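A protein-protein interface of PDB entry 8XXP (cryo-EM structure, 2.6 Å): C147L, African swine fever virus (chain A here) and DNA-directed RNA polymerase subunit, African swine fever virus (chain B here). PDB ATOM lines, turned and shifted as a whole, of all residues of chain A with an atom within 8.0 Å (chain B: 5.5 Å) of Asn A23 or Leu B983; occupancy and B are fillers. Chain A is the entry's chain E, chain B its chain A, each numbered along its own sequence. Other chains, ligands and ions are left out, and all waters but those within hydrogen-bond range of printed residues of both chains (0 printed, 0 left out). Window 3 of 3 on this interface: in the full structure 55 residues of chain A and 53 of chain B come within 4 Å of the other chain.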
ATOM      1  N   ILE A  20      25.149  16.288 -20.246  1.00  0.00           N
ATOM      2  CA  ILE A  20      25.304  14.903 -20.698  1.00  0.00           C
ATOM      3  C   ILE A  20      26.199  14.880 -21.928  1.00  0.00           C
ATOM      4  O   ILE A  20      26.012  15.707 -22.841  1.00  0.00           O
ATOM      5  CB  ILE A  20      23.929  14.290 -21.000  1.00  0.00           C
ATOM      6  CG1 ILE A  20      23.166  14.055 -19.703  1.00  0.00           C
ATOM      7  CG2 ILE A  20      24.064  13.001 -21.764  1.00  0.00           C
ATOM      8  CD1 ILE A  20      21.696  13.851 -19.899  1.00  0.00           C
ATOM      9  N   PRO A  21      27.181  13.983 -22.010  1.00  0.00           N
ATOM     10  CA  PRO A  21      28.087  13.983 -23.164  1.00  0.00           C
ATOM     11  C   PRO A  21      27.342  13.746 -24.468  1.00  0.00           C
ATOM     12  O   PRO A  21      26.295  13.100 -24.504  1.00  0.00           O
ATOM     13  CB  PRO A  21      29.053  12.836 -22.856  1.00  0.00           C
ATOM     14  CG  PRO A  21      28.994  12.682 -21.390  1.00  0.00           C
ATOM     15  CD  PRO A  21      27.605  13.023 -20.979  1.00  0.00           C
ATOM     16  N   ASP A  22      27.904  14.290 -25.550  1.00  0.00           N
ATOM     17  CA  ASP A  22      27.216  14.293 -26.836  1.00  0.00           C
ATOM     18  C   ASP A  22      26.870  12.889 -27.313  1.00  0.00           C
ATOM     19  O   ASP A  22      25.880  12.706 -28.025  1.00  0.00           O
ATOM     20  CB  ASP A  22      28.072  15.003 -27.882  1.00  0.00           C
ATOM     21  CG  ASP A  22      27.859  16.501 -27.889  1.00  0.00           C
ATOM     22  OD1 ASP A  22      26.978  16.983 -27.150  1.00  0.00           O
ATOM     23  OD2 ASP A  22      28.568  17.200 -28.641  1.00  0.00           O
ATOM     24  N   ASN A  23      27.667  11.892 -26.943  1.00  0.00           N
ATOM     25  CA  ASN A  23      27.385  10.529 -27.367  1.00  0.00           C
ATOM     26  C   ASN A  23      26.445   9.800 -26.422  1.00  0.00           C
ATOM     27  O   ASN A  23      26.068   8.659 -26.707  1.00  0.00           O
ATOM     28  CB  ASN A  23      28.687   9.748 -27.511  1.00  0.00           C
ATOM     29  CG  ASN A  23      29.254   9.826 -28.912  1.00  0.00           C
ATOM     30  OD1 ASN A  23      28.570  10.233 -29.846  1.00  0.00           O
ATOM     31  ND2 ASN A  23      30.512   9.439 -29.065  1.00  0.00           N
ATOM     32  N   GLU A  24      26.058  10.420 -25.313  1.00  0.00           N
ATOM     33  CA  GLU A  24      25.149   9.818 -24.355  1.00  0.00           C
ATOM     34  C   GLU A  24      23.751  10.406 -24.423  1.00  0.00           C
ATOM     35  O   GLU A  24      22.892  10.020 -23.629  1.00  0.00           O
ATOM     36  CB  GLU A  24      25.706   9.978 -22.941  1.00  0.00           C
ATOM     37  CG  GLU A  24      27.149   9.555 -22.807  1.00  0.00           C
ATOM     38  CD  GLU A  24      27.361   8.568 -21.691  1.00  0.00           C
ATOM     39  OE1 GLU A  24      27.307   8.982 -20.518  1.00  0.00           O
ATOM     40  OE2 GLU A  24      27.581   7.376 -21.986  1.00  0.00           O
ATOM     41  N   ARG A  25      23.506  11.326 -25.349  1.00  0.00           N
ATOM     42  CA  ARG A  25      22.214  11.984 -25.455  1.00  0.00           C
ATOM     43  C   ARG A  25      21.201  11.046 -26.090  1.00  0.00           C
ATOM     44  O   ARG A  25      21.483  10.426 -27.118  1.00  0.00           O
ATOM     45  CB  ARG A  25      22.343  13.262 -26.278  1.00  0.00           C
ATOM     46  CG  ARG A  25      23.273  14.292 -25.672  1.00  0.00           C
ATOM     47  CD  ARG A  25      23.345  15.526 -26.536  1.00  0.00           C
ATOM     48  NE  ARG A  25      23.960  15.250 -27.825  1.00  0.00           N
ATOM     49  CZ  ARG A  25      24.158  16.159 -28.768  1.00  0.00           C
ATOM     50  NH1 ARG A  25      23.794  17.417 -28.600  1.00  0.00           N
ATOM     51  NH2 ARG A  25      24.729  15.795 -29.910  1.00  0.00           N
ATOM     52  N   ILE A  26      20.019  10.947 -25.484  1.00  0.00           N
ATOM     53  CA  ILE A  26      18.966  10.065 -25.973  1.00  0.00           C
ATOM     54  C   ILE A  26      17.725  10.816 -26.422  1.00  0.00           C
ATOM     55  O   ILE A  26      16.767  10.184 -26.869  1.00  0.00           O
ATOM     56  CB  ILE A  26      18.590   8.997 -24.927  1.00  0.00           C
ATOM     57  CG1 ILE A  26      18.188   9.651 -23.611  1.00  0.00           C
ATOM     58  CG2 ILE A  26      19.736   8.030 -24.722  1.00  0.00           C
ATOM     59  CD1 ILE A  26      18.153   8.697 -22.459  1.00  0.00           C
ATOM     60  N   ASN B 978      19.656   9.683 -34.020  1.00  0.00           N
ATOM     61  CA  ASN B 978      20.621   9.043 -34.901  1.00  0.00           C
ATOM     62  C   ASN B 978      21.976   8.827 -34.238  1.00  0.00           C
ATOM     63  O   ASN B 978      22.793   8.075 -34.772  1.00  0.00           O
ATOM     64  CB  ASN B 978      20.777   9.871 -36.176  1.00  0.00           C
ATOM     65  CG  ASN B 978      21.473  11.194 -35.938  1.00  0.00           C
ATOM     66  OD1 ASN B 978      21.557  11.677 -34.812  1.00  0.00           O
ATOM     67  ND2 ASN B 978      21.965  11.796 -37.007  1.00  0.00           N
ATOM     68  N   ILE B 979      22.236   9.473 -33.101  1.00  0.00           N
ATOM     69  CA  ILE B 979      23.483   9.241 -32.378  1.00  0.00           C
ATOM     70  C   ILE B 979      23.504   7.838 -31.789  1.00  0.00           C
ATOM     71  O   ILE B 979      24.501   7.117 -31.889  1.00  0.00           O
ATOM     72  CB  ILE B 979      23.678  10.299 -31.280  1.00  0.00           C
ATOM     73  CG1 ILE B 979      23.692  11.701 -31.873  1.00  0.00           C
ATOM     74  CG2 ILE B 979      24.953  10.039 -30.515  1.00  0.00           C
ATOM     75  CD1 ILE B 979      23.827  12.772 -30.835  1.00  0.00           C
ATOM     76  N   GLN B 980      22.406   7.440 -31.145  1.00  0.00           N
ATOM     77  CA  GLN B 980      22.344   6.124 -30.527  1.00  0.00           C
ATOM     78  C   GLN B 980      22.200   5.026 -31.567  1.00  0.00           C
ATOM     79  O   GLN B 980      22.607   3.888 -31.324  1.00  0.00           O
ATOM     80  CB  GLN B 980      21.189   6.073 -29.534  1.00  0.00           C
ATOM     81  CG  GLN B 980      21.256   7.128 -28.447  1.00  0.00           C
ATOM     82  CD  GLN B 980      22.520   7.056 -27.633  1.00  0.00           C
ATOM     83  OE1 GLN B 980      23.489   7.754 -27.909  1.00  0.00           O
ATOM     84  NE2 GLN B 980      22.520   6.208 -26.622  1.00  0.00           N
ATOM     85  N   GLU B 981      21.613   5.342 -32.719  1.00  0.00           N
ATOM     86  CA  GLU B 981      21.583   4.383 -33.816  1.00  0.00           C
ATOM     87  C   GLU B 981      22.982   4.109 -34.344  1.00  0.00           C
ATOM     88  O   GLU B 981      23.335   2.957 -34.611  1.00  0.00           O
ATOM     89  CB  GLU B 981      20.682   4.902 -34.930  1.00  0.00           C
ATOM     90  CG  GLU B 981      20.377   3.889 -36.004  1.00  0.00           C
ATOM     91  CD  GLU B 981      19.510   4.463 -37.092  1.00  0.00           C
ATOM     92  OE1 GLU B 981      18.926   5.541 -36.868  1.00  0.00           O
ATOM     93  OE2 GLU B 981      19.410   3.846 -38.171  1.00  0.00           O
ATOM     94  N   ARG B 982      23.792   5.156 -34.496  1.00  0.00           N
ATOM     95  CA  ARG B 982      25.159   4.982 -34.968  1.00  0.00           C
ATOM     96  C   ARG B 982      25.978   4.144 -33.998  1.00  0.00           C
ATOM     97  O   ARG B 982      26.790   3.311 -34.415  1.00  0.00           O
ATOM     98  CB  ARG B 982      25.809   6.346 -35.181  1.00  0.00           C
ATOM     99  CG  ARG B 982      27.202   6.295 -35.761  1.00  0.00           C
ATOM    100  CD  ARG B 982      27.808   7.677 -35.803  1.00  0.00           C
ATOM    101  NE  ARG B 982      28.337   8.083 -34.509  1.00  0.00           N
ATOM    102  CZ  ARG B 982      27.879   9.104 -33.801  1.00  0.00           C
ATOM    103  NH1 ARG B 982      26.861   9.836 -34.222  1.00  0.00           N
ATOM    104  NH2 ARG B 982      28.457   9.400 -32.641  1.00  0.00           N
ATOM    105  N   LEU B 983      25.793   4.361 -32.700  1.00  0.00           N
ATOM    106  CA  LEU B 983      26.480   3.571 -31.692  1.00  0.00           C
ATOM    107  C   LEU B 983      25.803   2.236 -31.430  1.00  0.00           C
ATOM    108  O   LEU B 983      26.394   1.388 -30.754  1.00  0.00           O
ATOM    109  CB  LEU B 983      26.575   4.365 -30.391  1.00  0.00           C
ATOM    110  CG  LEU B 983      27.240   5.732 -30.519  1.00  0.00           C
ATOM    111  CD1 LEU B 983      27.345   6.400 -29.168  1.00  0.00           C
ATOM    112  CD2 LEU B 983      28.604   5.595 -31.153  1.00  0.00           C
ATOM    113  N   GLN B 984      24.588   2.038 -31.944  1.00  0.00           N
ATOM    114  CA  GLN B 984      23.838   0.791 -31.785  1.00  0.00           C
ATOM    115  C   GLN B 984      23.678   0.415 -30.315  1.00  0.00           C
ATOM    116  O   GLN B 984      23.797  -0.750 -29.937  1.00  0.00           O
ATOM    117  CB  GLN B 984      24.485  -0.345 -32.574  1.00  0.00           C
ATOM    118  CG  GLN B 984      24.289  -0.231 -34.070  1.00  0.00           C
ATOM    119  CD  GLN B 984      22.864  -0.497 -34.485  1.00  0.00           C
ATOM    120  OE1 GLN B 984      22.224  -1.411 -33.980  1.00  0.00           O
ATOM    121  NE2 GLN B 984      22.354   0.307 -35.402  1.00  0.00           N
ATOM    122  N   THR B 985      23.402   1.414 -29.484  1.00  0.00           N
ATOM    123  CA  THR B 985      23.156   1.187 -28.074  1.00  0.00           C
ATOM    124  C   THR B 985      21.826   0.460 -27.891  1.00  0.00           C
ATOM    125  O   THR B 985      20.972   0.482 -28.779  1.00  0.00           O
ATOM    126  CB  THR B 985      23.151   2.514 -27.323  1.00  0.00           C
ATOM    127  OG1 THR B 985      22.130   3.362 -27.854  1.00  0.00           O
ATOM    128  CG2 THR B 985      24.491   3.205 -27.469  1.00  0.00           C
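The side-chain amide oxygen of Gln B980 lies close to the backbone carbonyl oxygen of Asn A23, at 3.0 Å.
O of Arg A25 sits close to OE1 of Gln B980 (3.4 Å).
The guanidinium group of Arg B982 is in hydrogen-bond range of the side-chain amide oxygen of Asn A23.
The side-chain amide nitrogen (NE2) of Gln B980 is in hydrogen-bond range of the side-chain hydroxyl (OG1) of Thr B985, at 3.1 Å.
The guanidinium group of Arg A25 lies within salt-bridge range of the side-chain carboxylate of Asp A22 (3.5 Å).
Asp A22 touches Ile B979.
Asn A23 touches Ile B979 (OD1 to CG2, 3.7 Å).
O of Asn A23 touches CD1 of Leu B983 (3.6 Å).
Ile B979 touches Arg A25 (CD1 to NH2, 3.3 Å).
Gln B980 touches Ile A26 (NE2 to CG2, 3.8 Å).
Asn A23 touches just these residues of chain B: Ile B979, Gln B980, Arg B982 and Leu B983.
Of chain A, only Asn A23 (3.6 Å) comes within 4 Å of Leu B983.
Printed residues of chain A within 4 Å of Gln B980: Asn A23, Arg A25 and Ile A26.
Printed residues of chain A within 4 Å of Arg B982: Asn A23 (2.9 Å).
Printed residues of chain B within 4 Å of Ile A26: Gln B980 (3.8 Å).
Printed residues of chain B within 4 Å of Arg A25: Ile B979 (3.3 Å) and Gln B980 (3.4 Å).
Of the printed residues of chain A, Ile B979 touches Asp A22 (3.5 Å), Asn A23 (3.7 Å) and Arg A25 (3.3 Å).
Glu B981 touches none of the printed residues of chain A.
The nearest printed residue of chain B that does not touch Asn A23 is Thr B985 (5.7 Å).
The nearest residue of chain A that does not touch Leu B983 is Glu A24 (5.7 Å).
Of the 7 printed residues of chain A, 4 touch a printed residue of chain B.
Hydrophobic or aromatic side chains of chain A that line the printed part of chain B: Ile A26.
Of the 8 printed residues of chain B, 4 touch a printed residue of chain A.
Printed residues of chain B that touch a printed residue of chain A: Ile B979, Gln B980, Arg B982 and Leu B983.
Hydrophobic or aromatic side chains of chain B that line the printed part of chain A: Ile B979 and Leu B983.
Among the printed residues, 8 pairs touch across the chains.
Among the printed residues, no Asp or Glu carboxylate lies within 4 Å of a Lys or Arg side-chain nitrogen of the other chain.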
